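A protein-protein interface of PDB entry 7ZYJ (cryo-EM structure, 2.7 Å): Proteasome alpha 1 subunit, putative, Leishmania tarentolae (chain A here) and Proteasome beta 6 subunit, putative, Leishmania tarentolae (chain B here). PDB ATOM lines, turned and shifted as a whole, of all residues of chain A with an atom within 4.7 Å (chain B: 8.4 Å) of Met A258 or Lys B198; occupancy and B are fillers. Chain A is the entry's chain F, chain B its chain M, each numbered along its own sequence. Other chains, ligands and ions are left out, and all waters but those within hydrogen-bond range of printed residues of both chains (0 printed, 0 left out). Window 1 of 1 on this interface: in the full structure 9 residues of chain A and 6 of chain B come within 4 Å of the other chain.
The side-chain amide oxygen (OD1) of Asn A259 lies close to the backbone carbonyl oxygen (O) of Thr A255 (3.2 Å). The side-chain carboxylate (OD2) of Asp A232 is in salt-bridge range of the guanidinium group (NH2) of Arg A261 (2.5 Å). The backbone carbonyl oxygen of Trp B199 lies close to the side-chain amide nitrogen of Asn B203 (3.3 Å).
Of the 11 printed residues of chain A, 7 touch a printed residue of chain B. Hydrophobic or aromatic side chains of chain A that line the printed part of chain B: Met A258 and Tyr A262. Along chain A the printed residues that touch a printed residue of chain B span positions 231 to 262. Of the 22 printed residues of chain B, 5 touch a printed residue of chain A. Among the printed residues, Asp or Glu carboxylates within 4 Å of a Lys or Arg side-chain nitrogen of the other chain: Asp A232 with Lys B198 (2.5 Å).
The side-chain sulfur of Met A258 sits at hydrogen-bond distance from the indole nitrogen of Trp B199, at 3.4 Å. The side-chain hydroxyl of Tyr B195 sits at hydrogen-bond distance from the backbone NH of Tyr A262, at 3.0 Å. NZ of Lys B198 is in salt-bridge range of OD1 of Asp A232 (2.5 Å). OH of Tyr B202 sits at hydrogen-bond distance from O of Ile A231, at 3.1 Å. The side-chain hydroxyl (OH) of Tyr B195 sits at hydrogen-bond distance from the backbone carbonyl oxygen (O) of Met A258.
Tyr B202 touches Asp A232. Arg A254 touches Trp B199 (CB to CH2, 3.7 Å). Arg A254 touches Tyr B202 (NH2 to CD1, 3.6 Å). Thr A255 touches Trp B199 (OG1 to CZ2, 3.4 Å). CD of Lys B198 touches CE of Met A258, at 3.8 Å. Met A258 touches Tyr B202. Tyr B195 touches Arg A261. CD1 of Tyr A262 touches CG of Gln B191 (3.9 Å).
Met A258 touches just these residues of chain B: Tyr B195 (3.2 Å), Lys B198 (3.8 Å), Trp B199 (3.4 Å) and Tyr B202 (3.8 Å). Lys B198 touches just these residues of chain A: Asp A232 and Met A258. Of the printed residues of chain B, Thr A255 touches Trp B199. Of the printed residues of chain B, Arg A254 touches Trp B199 (3.7 Å) and Tyr B202 (3.6 Å). Printed residues of chain B within 4 Å of Tyr A262: Gln B191 and Tyr B195. Of the printed residues of chain B, Asp A232 touches Lys B198 and Tyr B202. Leu B171 touches none of the printed residues of chain A. Pro B209 touches none of the printed residues of chain A. The nearest printed residue of chain B that does not touch Asp A232 is Tyr B195 (6.4 Å).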
ATOM      1  N   ILE A 231      27.648 -23.395 -20.805  1.00  0.00           N
ATOM      2  CA  ILE A 231      26.553 -22.510 -20.432  1.00  0.00           C
ATOM      3  C   ILE A 231      26.489 -21.284 -21.332  1.00  0.00           C
ATOM      4  O   ILE A 231      25.404 -20.860 -21.731  1.00  0.00           O
ATOM      5  CB  ILE A 231      26.683 -22.105 -18.948  1.00  0.00           C
ATOM      6  CG1 ILE A 231      26.718 -23.347 -18.058  1.00  0.00           C
ATOM      7  CG2 ILE A 231      25.536 -21.202 -18.540  1.00  0.00           C
ATOM      8  CD1 ILE A 231      25.528 -24.261 -18.239  1.00  0.00           C
ATOM      9  N   ASP A 232      27.639 -20.710 -21.665  1.00  0.00           N
ATOM     10  CA  ASP A 232      27.713 -19.529 -22.514  1.00  0.00           C
ATOM     11  C   ASP A 232      29.118 -19.477 -23.103  1.00  0.00           C
ATOM     12  O   ASP A 232      29.962 -20.326 -22.802  1.00  0.00           O
ATOM     13  CB  ASP A 232      27.362 -18.265 -21.722  1.00  0.00           C
ATOM     14  CG  ASP A 232      26.903 -17.127 -22.612  1.00  0.00           C
ATOM     15  OD1 ASP A 232      25.877 -17.285 -23.304  1.00  0.00           O
ATOM     16  OD2 ASP A 232      27.569 -16.071 -22.617  1.00  0.00           O
ATOM     17  N   ARG A 254      21.575 -21.670 -18.887  1.00  0.00           N
ATOM     18  CA  ARG A 254      21.626 -21.269 -20.288  1.00  0.00           C
ATOM     19  C   ARG A 254      20.543 -20.249 -20.607  1.00  0.00           C
ATOM     20  O   ARG A 254      20.791 -19.275 -21.328  1.00  0.00           O
ATOM     21  CB  ARG A 254      21.496 -22.496 -21.187  1.00  0.00           C
ATOM     22  CG  ARG A 254      22.745 -23.354 -21.236  1.00  0.00           C
ATOM     23  CD  ARG A 254      22.416 -24.778 -21.637  1.00  0.00           C
ATOM     24  NE  ARG A 254      23.611 -25.531 -21.996  1.00  0.00           N
ATOM     25  CZ  ARG A 254      23.614 -26.815 -22.326  1.00  0.00           C
ATOM     26  NH1 ARG A 254      22.498 -27.524 -22.351  1.00  0.00           N
ATOM     27  NH2 ARG A 254      24.765 -27.401 -22.639  1.00  0.00           N
ATOM     28  N   THR A 255      19.332 -20.451 -20.076  1.00  0.00           N
ATOM     29  CA  THR A 255      18.263 -19.485 -20.303  1.00  0.00           C
ATOM     30  C   THR A 255      18.613 -18.126 -19.711  1.00  0.00           C
ATOM     31  O   THR A 255      18.396 -17.088 -20.347  1.00  0.00           O
ATOM     32  CB  THR A 255      16.952 -20.004 -19.716  1.00  0.00           C
ATOM     33  OG1 THR A 255      16.691 -21.321 -20.217  1.00  0.00           O
ATOM     34  CG2 THR A 255      15.799 -19.089 -20.096  1.00  0.00           C
ATOM     35  N   GLU A 256      19.165 -18.112 -18.495  1.00  0.00           N
ATOM     36  CA  GLU A 256      19.528 -16.845 -17.868  1.00  0.00           C
ATOM     37  C   GLU A 256      20.656 -16.152 -18.623  1.00  0.00           C
ATOM     38  O   GLU A 256      20.641 -14.926 -18.782  1.00  0.00           O
ATOM     39  CB  GLU A 256      19.914 -17.071 -16.407  1.00  0.00           C
ATOM     40  CG  GLU A 256      18.780 -17.598 -15.542  1.00  0.00           C
ATOM     41  CD  GLU A 256      17.525 -16.752 -15.633  1.00  0.00           C
ATOM     42  OE1 GLU A 256      17.638 -15.510 -15.689  1.00  0.00           O
ATOM     43  OE2 GLU A 256      16.419 -17.331 -15.652  1.00  0.00           O
ATOM     44  N   CYS A 257      21.640 -16.918 -19.095  1.00  0.00           N
ATOM     45  CA  CYS A 257      22.723 -16.334 -19.881  1.00  0.00           C
ATOM     46  C   CYS A 257      22.206 -15.752 -21.187  1.00  0.00           C
ATOM     47  O   CYS A 257      22.632 -14.668 -21.602  1.00  0.00           O
ATOM     48  CB  CYS A 257      23.793 -17.386 -20.159  1.00  0.00           C
ATOM     49  SG  CYS A 257      24.882 -17.705 -18.774  1.00  0.00           S
ATOM     50  N   MET A 258      21.296 -16.462 -21.854  1.00  0.00           N
ATOM     51  CA  MET A 258      20.718 -15.951 -23.090  1.00  0.00           C
ATOM     52  C   MET A 258      19.919 -14.681 -22.834  1.00  0.00           C
ATOM     53  O   MET A 258      19.975 -13.735 -23.629  1.00  0.00           O
ATOM     54  CB  MET A 258      19.842 -17.023 -23.736  1.00  0.00           C
ATOM     55  CG  MET A 258      20.612 -18.016 -24.585  1.00  0.00           C
ATOM     56  SD  MET A 258      19.547 -19.243 -25.363  1.00  0.00           S
ATOM     57  CE  MET A 258      20.572 -20.705 -25.228  1.00  0.00           C
ATOM     58  N   ASN A 259      19.164 -14.644 -21.734  1.00  0.00           N
ATOM     59  CA  ASN A 259      18.415 -13.440 -21.390  1.00  0.00           C
ATOM     60  C   ASN A 259      19.347 -12.265 -21.121  1.00  0.00           C
ATOM     61  O   ASN A 259      19.090 -11.145 -21.576  1.00  0.00           O
ATOM     62  CB  ASN A 259      17.526 -13.703 -20.174  1.00  0.00           C
ATOM     63  CG  ASN A 259      16.326 -14.570 -20.502  1.00  0.00           C
ATOM     64  OD1 ASN A 259      16.206 -15.087 -21.612  1.00  0.00           O
ATOM     65  ND2 ASN A 259      15.432 -14.739 -19.535  1.00  0.00           N
ATOM     66  N   TYR A 260      20.433 -12.501 -20.383  1.00  0.00           N
ATOM     67  CA  TYR A 260      21.354 -11.416 -20.055  1.00  0.00           C
ATOM     68  C   TYR A 260      22.064 -10.899 -21.299  1.00  0.00           C
ATOM     69  O   TYR A 260      22.133  -9.687 -21.526  1.00  0.00           O
ATOM     70  CB  TYR A 260      22.367 -11.881 -19.009  1.00  0.00           C
ATOM     71  CG  TYR A 260      23.274 -10.783 -18.498  1.00  0.00           C
ATOM     72  CD1 TYR A 260      24.409 -10.405 -19.201  1.00  0.00           C
ATOM     73  CD2 TYR A 260      22.993 -10.123 -17.308  1.00  0.00           C
ATOM     74  CE1 TYR A 260      25.235  -9.401 -18.739  1.00  0.00           C
ATOM     75  CE2 TYR A 260      23.816  -9.119 -16.838  1.00  0.00           C
ATOM     76  CZ  TYR A 260      24.936  -8.763 -17.558  1.00  0.00           C
ATOM     77  OH  TYR A 260      25.760  -7.764 -17.096  1.00  0.00           O
ATOM     78  N   ARG A 261      22.613 -11.806 -22.113  1.00  0.00           N
ATOM     79  CA  ARG A 261      23.328 -11.385 -23.310  1.00  0.00           C
ATOM     80  C   ARG A 261      22.414 -10.681 -24.303  1.00  0.00           C
ATOM     81  O   ARG A 261      22.894  -9.898 -25.127  1.00  0.00           O
ATOM     82  CB  ARG A 261      23.999 -12.586 -23.973  1.00  0.00           C
ATOM     83  CG  ARG A 261      25.067 -12.216 -24.988  1.00  0.00           C
ATOM     84  CD  ARG A 261      25.764 -13.446 -25.535  1.00  0.00           C
ATOM     85  NE  ARG A 261      26.736 -13.990 -24.595  1.00  0.00           N
ATOM     86  CZ  ARG A 261      27.968 -13.525 -24.438  1.00  0.00           C
ATOM     87  NH1 ARG A 261      28.411 -12.492 -25.134  1.00  0.00           N
ATOM     88  NH2 ARG A 261      28.775 -14.112 -23.560  1.00  0.00           N
ATOM     89  N   TYR A 262      21.108 -10.941 -24.241  1.00  0.00           N
ATOM     90  CA  TYR A 262      20.173 -10.226 -25.099  1.00  0.00           C
ATOM     91  C   TYR A 262      19.960  -8.795 -24.623  1.00  0.00           C
ATOM     92  O   TYR A 262      19.874  -7.877 -25.446  1.00  0.00           O
ATOM     93  CB  TYR A 262      18.845 -10.984 -25.156  1.00  0.00           C
ATOM     94  CG  TYR A 262      17.686 -10.183 -25.698  1.00  0.00           C
ATOM     95  CD1 TYR A 262      17.529  -9.991 -27.063  1.00  0.00           C
ATOM     96  CD2 TYR A 262      16.738  -9.635 -24.846  1.00  0.00           C
ATOM     97  CE1 TYR A 262      16.470  -9.264 -27.562  1.00  0.00           C
ATOM     98  CE2 TYR A 262      15.675  -8.907 -25.337  1.00  0.00           C
ATOM     99  CZ  TYR A 262      15.545  -8.725 -26.695  1.00  0.00           C
ATOM    100  OH  TYR A 262      14.486  -8.000 -27.186  1.00  0.00           O
ATOM    101  N   LEU B 171      24.637 -16.450 -38.816  1.00  0.00           N
ATOM    102  CA  LEU B 171      24.012 -17.395 -37.902  1.00  0.00           C
ATOM    103  C   LEU B 171      24.944 -18.558 -37.580  1.00  0.00           C
ATOM    104  O   LEU B 171      25.133 -18.905 -36.410  1.00  0.00           O
ATOM    105  CB  LEU B 171      22.700 -17.907 -38.499  1.00  0.00           C
ATOM    106  CG  LEU B 171      21.617 -16.839 -38.647  1.00  0.00           C
ATOM    107  CD1 LEU B 171      20.536 -17.287 -39.616  1.00  0.00           C
ATOM    108  CD2 LEU B 171      21.028 -16.497 -37.293  1.00  0.00           C
ATOM    109  N   THR B 172      25.524 -19.165 -38.604  1.00  0.00           N
ATOM    110  CA  THR B 172      26.530 -20.209 -38.488  1.00  0.00           C
ATOM    111  C   THR B 172      27.675 -19.864 -39.420  1.00  0.00           C
ATOM    112  O   THR B 172      27.537 -19.011 -40.301  1.00  0.00           O
ATOM    113  CB  THR B 172      25.952 -21.592 -38.842  1.00  0.00           C
ATOM    114  OG1 THR B 172      25.869 -21.731 -40.265  1.00  0.00           O
ATOM    115  CG2 THR B 172      24.578 -21.782 -38.230  1.00  0.00           C
ATOM    116  N   GLN B 191      18.222 -11.707 -33.176  1.00  0.00           N
ATOM    117  CA  GLN B 191      18.420 -12.250 -31.836  1.00  0.00           C
ATOM    118  C   GLN B 191      17.651 -13.555 -31.646  1.00  0.00           C
ATOM    119  O   GLN B 191      18.183 -14.521 -31.078  1.00  0.00           O
ATOM    120  CB  GLN B 191      18.005 -11.222 -30.786  1.00  0.00           C
ATOM    121  CG  GLN B 191      18.888  -9.992 -30.767  1.00  0.00           C
ATOM    122  CD  GLN B 191      20.324 -10.319 -30.417  1.00  0.00           C
ATOM    123  OE1 GLN B 191      20.600 -10.901 -29.370  1.00  0.00           O
ATOM    124  NE2 GLN B 191      21.247  -9.950 -31.296  1.00  0.00           N
ATOM    125  N   MET B 192      16.404 -13.603 -32.120  1.00  0.00           N
ATOM    126  CA  MET B 192      15.608 -14.821 -31.983  1.00  0.00           C
ATOM    127  C   MET B 192      16.227 -15.982 -32.755  1.00  0.00           C
ATOM    128  O   MET B 192      16.317 -17.104 -32.241  1.00  0.00           O
ATOM    129  CB  MET B 192      14.174 -14.558 -32.441  1.00  0.00           C
ATOM    130  CG  MET B 192      13.420 -13.567 -31.566  1.00  0.00           C
ATOM    131  SD  MET B 192      13.223 -14.145 -29.866  1.00  0.00           S
ATOM    132  CE  MET B 192      14.483 -13.211 -29.001  1.00  0.00           C
ATOM    133  N   LEU B 193      16.666 -15.732 -33.993  1.00  0.00           N
ATOM    134  CA  LEU B 193      17.334 -16.776 -34.765  1.00  0.00           C
ATOM    135  C   LEU B 193      18.608 -17.247 -34.078  1.00  0.00           C
ATOM    136  O   LEU B 193      18.877 -18.452 -34.019  1.00  0.00           O
ATOM    137  CB  LEU B 193      17.657 -16.285 -36.178  1.00  0.00           C
ATOM    138  CG  LEU B 193      16.666 -16.457 -37.334  1.00  0.00           C
ATOM    139  CD1 LEU B 193      16.414 -17.935 -37.601  1.00  0.00           C
ATOM    140  CD2 LEU B 193      15.369 -15.716 -37.110  1.00  0.00           C
ATOM    141  N   LYS B 194      19.409 -16.312 -33.563  1.00  0.00           N
ATOM    142  CA  LYS B 194      20.662 -16.684 -32.915  1.00  0.00           C
ATOM    143  C   LYS B 194      20.412 -17.564 -31.701  1.00  0.00           C
ATOM    144  O   LYS B 194      21.093 -18.580 -31.506  1.00  0.00           O
ATOM    145  CB  LYS B 194      21.433 -15.425 -32.520  1.00  0.00           C
ATOM    146  CG  LYS B 194      22.592 -15.670 -31.574  1.00  0.00           C
ATOM    147  CD  LYS B 194      23.144 -14.360 -31.042  1.00  0.00           C
ATOM    148  CE  LYS B 194      24.299 -14.596 -30.086  1.00  0.00           C
ATOM    149  NZ  LYS B 194      24.906 -13.315 -29.632  1.00  0.00           N
ATOM    150  N   TYR B 195      19.422 -17.209 -30.884  1.00  0.00           N
ATOM    151  CA  TYR B 195      19.168 -18.004 -29.690  1.00  0.00           C
ATOM    152  C   TYR B 195      18.518 -19.343 -30.017  1.00  0.00           C
ATOM    153  O   TYR B 195      18.802 -20.339 -29.342  1.00  0.00           O
ATOM    154  CB  TYR B 195      18.331 -17.198 -28.699  1.00  0.00           C
ATOM    155  CG  TYR B 195      19.130 -16.074 -28.084  1.00  0.00           C
ATOM    156  CD1 TYR B 195      20.435 -16.288 -27.660  1.00  0.00           C
ATOM    157  CD2 TYR B 195      18.596 -14.800 -27.945  1.00  0.00           C
ATOM    158  CE1 TYR B 195      21.182 -15.272 -27.104  1.00  0.00           C
ATOM    159  CE2 TYR B 195      19.338 -13.775 -27.389  1.00  0.00           C
ATOM    160  CZ  TYR B 195      20.631 -14.018 -26.971  1.00  0.00           C
ATOM    161  OH  TYR B 195      21.379 -13.007 -26.416  1.00  0.00           O
ATOM    162  N   ARG B 196      17.678 -19.404 -31.053  1.00  0.00           N
ATOM    163  CA  ARG B 196      17.152 -20.695 -31.487  1.00  0.00           C
ATOM    164  C   ARG B 196      18.264 -21.597 -32.010  1.00  0.00           C
ATOM    165  O   ARG B 196      18.270 -22.805 -31.748  1.00  0.00           O
ATOM    166  CB  ARG B 196      16.074 -20.495 -32.548  1.00  0.00           C
ATOM    167  CG  ARG B 196      14.765 -19.977 -31.993  1.00  0.00           C
ATOM    168  CD  ARG B 196      14.146 -20.964 -31.022  1.00  0.00           C
ATOM    169  NE  ARG B 196      13.683 -22.170 -31.696  1.00  0.00           N
ATOM    170  CZ  ARG B 196      12.452 -22.345 -32.156  1.00  0.00           C
ATOM    171  NH1 ARG B 196      11.529 -21.407 -32.030  1.00  0.00           N
ATOM    172  NH2 ARG B 196      12.140 -23.488 -32.758  1.00  0.00           N
ATOM    173  N   VAL B 197      19.217 -21.028 -32.751  1.00  0.00           N
ATOM    174  CA  VAL B 197      20.347 -21.810 -33.246  1.00  0.00           C
ATOM    175  C   VAL B 197      21.199 -22.308 -32.087  1.00  0.00           C
ATOM    176  O   VAL B 197      21.669 -23.453 -32.089  1.00  0.00           O
ATOM    177  CB  VAL B 197      21.170 -20.973 -34.243  1.00  0.00           C
ATOM    178  CG1 VAL B 197      22.531 -21.605 -34.484  1.00  0.00           C
ATOM    179  CG2 VAL B 197      20.418 -20.825 -35.554  1.00  0.00           C
ATOM    180  N   LYS B 198      21.415 -21.462 -31.079  1.00  0.00           N
ATOM    181  CA  LYS B 198      22.195 -21.880 -29.919  1.00  0.00           C
ATOM    182  C   LYS B 198      21.483 -22.985 -29.142  1.00  0.00           C
ATOM    183  O   LYS B 198      22.121 -23.937 -28.674  1.00  0.00           O
ATOM    184  CB  LYS B 198      22.477 -20.666 -29.035  1.00  0.00           C
ATOM    185  CG  LYS B 198      23.376 -20.927 -27.846  1.00  0.00           C
ATOM    186  CD  LYS B 198      23.645 -19.627 -27.105  1.00  0.00           C
ATOM    187  CE  LYS B 198      24.539 -19.842 -25.901  1.00  0.00           C
ATOM    188  NZ  LYS B 198      24.803 -18.573 -25.171  1.00  0.00           N
ATOM    189  N   TRP B 199      20.157 -22.884 -29.008  1.00  0.00           N
ATOM    190  CA  TRP B 199      19.393 -23.956 -28.377  1.00  0.00           C
ATOM    191  C   TRP B 199      19.482 -25.249 -29.179  1.00  0.00           C
ATOM    192  O   TRP B 199      19.591 -26.337 -28.603  1.00  0.00           O
ATOM    193  CB  TRP B 199      17.932 -23.536 -28.207  1.00  0.00           C
ATOM    194  CG  TRP B 199      17.632 -22.835 -26.914  1.00  0.00           C
ATOM    195  CD1 TRP B 199      16.959 -21.659 -26.763  1.00  0.00           C
ATOM    196  CD2 TRP B 199      17.970 -23.275 -25.591  1.00  0.00           C
ATOM    197  NE1 TRP B 199      16.867 -21.333 -25.433  1.00  0.00           N
ATOM    198  CE2 TRP B 199      17.479 -22.309 -24.692  1.00  0.00           C
ATOM    199  CE3 TRP B 199      18.642 -24.390 -25.079  1.00  0.00           C
ATOM    200  CZ2 TRP B 199      17.640 -22.420 -23.314  1.00  0.00           C
ATOM    201  CZ3 TRP B 199      18.801 -24.498 -23.710  1.00  0.00           C
ATOM    202  CH2 TRP B 199      18.302 -23.520 -22.845  1.00  0.00           C
ATOM    203  N   TYR B 200      19.420 -25.151 -30.508  1.00  0.00           N
ATOM    204  CA  TYR B 200      19.572 -26.332 -31.351  1.00  0.00           C
ATOM    205  C   TYR B 200      20.937 -26.973 -31.144  1.00  0.00           C
ATOM    206  O   TYR B 200      21.057 -28.200 -31.066  1.00  0.00           O
ATOM    207  CB  TYR B 200      19.363 -25.954 -32.820  1.00  0.00           C
ATOM    208  CG  TYR B 200      19.491 -27.102 -33.802  1.00  0.00           C
ATOM    209  CD1 TYR B 200      20.735 -27.529 -34.248  1.00  0.00           C
ATOM    210  CD2 TYR B 200      18.365 -27.753 -34.285  1.00  0.00           C
ATOM    211  CE1 TYR B 200      20.853 -28.574 -35.140  1.00  0.00           C
ATOM    212  CE2 TYR B 200      18.474 -28.799 -35.179  1.00  0.00           C
ATOM    213  CZ  TYR B 200      19.721 -29.204 -35.603  1.00  0.00           C
ATOM    214  OH  TYR B 200      19.837 -30.244 -36.494  1.00  0.00           O
ATOM    215  N   LYS B 201      21.982 -26.150 -31.063  1.00  0.00           N
ATOM    216  CA  LYS B 201      23.324 -26.673 -30.826  1.00  0.00           C
ATOM    217  C   LYS B 201      23.409 -27.370 -29.474  1.00  0.00           C
ATOM    218  O   LYS B 201      24.046 -28.422 -29.348  1.00  0.00           O
ATOM    219  CB  LYS B 201      24.347 -25.542 -30.920  1.00  0.00           C
ATOM    220  CG  LYS B 201      25.733 -25.909 -30.424  1.00  0.00           C
ATOM    221  CD  LYS B 201      26.761 -24.879 -30.854  1.00  0.00           C
ATOM    222  CE  LYS B 201      26.864 -24.802 -32.367  1.00  0.00           C
ATOM    223  NZ  LYS B 201      27.918 -23.846 -32.803  1.00  0.00           N
ATOM    224  N   TYR B 202      22.774 -26.796 -28.451  1.00  0.00           N
ATOM    225  CA  TYR B 202      22.749 -27.442 -27.141  1.00  0.00           C
ATOM    226  C   TYR B 202      21.999 -28.768 -27.178  1.00  0.00           C
ATOM    227  O   TYR B 202      22.424 -29.745 -26.551  1.00  0.00           O
ATOM    228  CB  TYR B 202      22.125 -26.510 -26.103  1.00  0.00           C
ATOM    229  CG  TYR B 202      23.044 -25.403 -25.654  1.00  0.00           C
ATOM    230  CD1 TYR B 202      24.418 -25.577 -25.669  1.00  0.00           C
ATOM    231  CD2 TYR B 202      22.539 -24.192 -25.204  1.00  0.00           C
ATOM    232  CE1 TYR B 202      25.265 -24.578 -25.257  1.00  0.00           C
ATOM    233  CE2 TYR B 202      23.382 -23.182 -24.788  1.00  0.00           C
ATOM    234  CZ  TYR B 202      24.745 -23.382 -24.816  1.00  0.00           C
ATOM    235  OH  TYR B 202      25.598 -22.386 -24.403  1.00  0.00           O
ATOM    236  N   ASN B 203      20.880 -28.823 -27.901  1.00  0.00           N
ATOM    237  CA  ASN B 203      20.023 -30.001 -27.879  1.00  0.00           C
ATOM    238  C   ASN B 203      20.465 -31.084 -28.855  1.00  0.00           C
ATOM    239  O   ASN B 203      19.873 -32.169 -28.859  1.00  0.00           O
ATOM    240  CB  ASN B 203      18.577 -29.605 -28.180  1.00  0.00           C
ATOM    241  CG  ASN B 203      17.948 -28.803 -27.060  1.00  0.00           C
ATOM    242  OD1 ASN B 203      18.357 -28.905 -25.905  1.00  0.00           O
ATOM    243  ND2 ASN B 203      16.950 -27.997 -27.398  1.00  0.00           N
ATOM    244  N   ASN B 204      21.477 -30.827 -29.676  1.00  0.00           N
ATOM    245  CA  ASN B 204      21.934 -31.779 -30.681  1.00  0.00           C
ATOM    246  C   ASN B 204      23.420 -32.081 -30.523  1.00  0.00           C
ATOM    247  O   ASN B 204      24.113 -32.403 -31.490  1.00  0.00           O
ATOM    248  CB  ASN B 204      21.631 -31.268 -32.087  1.00  0.00           C
ATOM    249  CG  ASN B 204      20.164 -31.395 -32.447  1.00  0.00           C
ATOM    250  OD1 ASN B 204      19.343 -30.565 -32.059  1.00  0.00           O
ATOM    251  ND2 ASN B 204      19.827 -32.440 -33.194  1.00  0.00           N
ATOM    252  N   GLY B 205      23.921 -31.986 -29.295  1.00  0.00           N
ATOM    253  CA  GLY B 205      25.302 -32.335 -29.018  1.00  0.00           C
ATOM    254  C   GLY B 205      26.331 -31.484 -29.726  1.00  0.00           C
ATOM    255  O   GLY B 205      27.347 -32.012 -30.190  1.00  0.00           O
ATOM    256  N   GLY B 206      26.102 -30.177 -29.822  1.00  0.00           N
ATOM    257  CA  GLY B 206      27.041 -29.298 -30.484  1.00  0.00           C
ATOM    258  C   GLY B 206      26.994 -29.325 -31.993  1.00  0.00           C
ATOM    259  O   GLY B 206      27.854 -28.709 -32.633  1.00  0.00           O
ATOM    260  N   LYS B 207      26.022 -30.014 -32.584  1.00  0.00           N
ATOM    261  CA  LYS B 207      25.902 -30.080 -34.033  1.00  0.00           C
ATOM    262  C   LYS B 207      25.258 -28.794 -34.538  1.00  0.00           C
ATOM    263  O   LYS B 207      24.149 -28.442 -34.122  1.00  0.00           O
ATOM    264  CB  LYS B 207      25.089 -31.311 -34.437  1.00  0.00           C
ATOM    265  CG  LYS B 207      25.032 -31.600 -35.933  1.00  0.00           C
ATOM    266  CD  LYS B 207      23.838 -30.938 -36.604  1.00  0.00           C
ATOM    267  CE  LYS B 207      23.762 -31.303 -38.076  1.00  0.00           C
ATOM    268  NZ  LYS B 207      22.620 -30.633 -38.756  1.00  0.00           N
ATOM    269  N   VAL B 208      25.953 -28.094 -35.424  1.00  0.00           N
ATOM    270  CA  VAL B 208      25.450 -26.814 -35.935  1.00  0.00           C
ATOM    271  C   VAL B 208      24.343 -27.078 -36.951  1.00  0.00           C
ATOM    272  O   VAL B 208      24.455 -28.023 -37.753  1.00  0.00           O
ATOM    273  CB  VAL B 208      26.600 -25.995 -36.542  1.00  0.00           C
ATOM    274  CG1 VAL B 208      27.020 -26.521 -37.912  1.00  0.00           C
ATOM    275  CG2 VAL B 208      26.247 -24.522 -36.609  1.00  0.00           C
ATOM    276  N   PRO B 209      23.244 -26.327 -36.928  1.00  0.00           N
ATOM    277  CA  PRO B 209      22.165 -26.573 -37.889  1.00  0.00           C
ATOM    278  C   PRO B 209      22.586 -26.250 -39.314  1.00  0.00           C
ATOM    279  O   PRO B 209      23.426 -25.384 -39.570  1.00  0.00           O
ATOM    280  CB  PRO B 209      21.042 -25.640 -37.419  1.00  0.00           C
ATOM    281  CG  PRO B 209      21.724 -24.599 -36.605  1.00  0.00           C
ATOM    282  CD  PRO B 209      22.889 -25.279 -35.957  1.00  0.00           C
ATOM    283  N   LEU B 217      13.286 -23.131 -40.046  1.00  0.00           N
ATOM    284  CA  LEU B 217      13.069 -22.475 -38.761  1.00  0.00           C
ATOM    285  C   LEU B 217      12.687 -21.012 -38.945  1.00  0.00           C
ATOM    286  O   LEU B 217      11.808 -20.499 -38.242  1.00  0.00           O
ATOM    287  CB  LEU B 217      14.320 -22.603 -37.893  1.00  0.00           C
ATOM    288  CG  LEU B 217      14.411 -21.696 -36.665  1.00  0.00           C
ATOM    289  CD1 LEU B 217      13.332 -22.044 -35.656  1.00  0.00           C
ATOM    290  CD2 LEU B 217      15.789 -21.794 -36.034  1.00  0.00           C
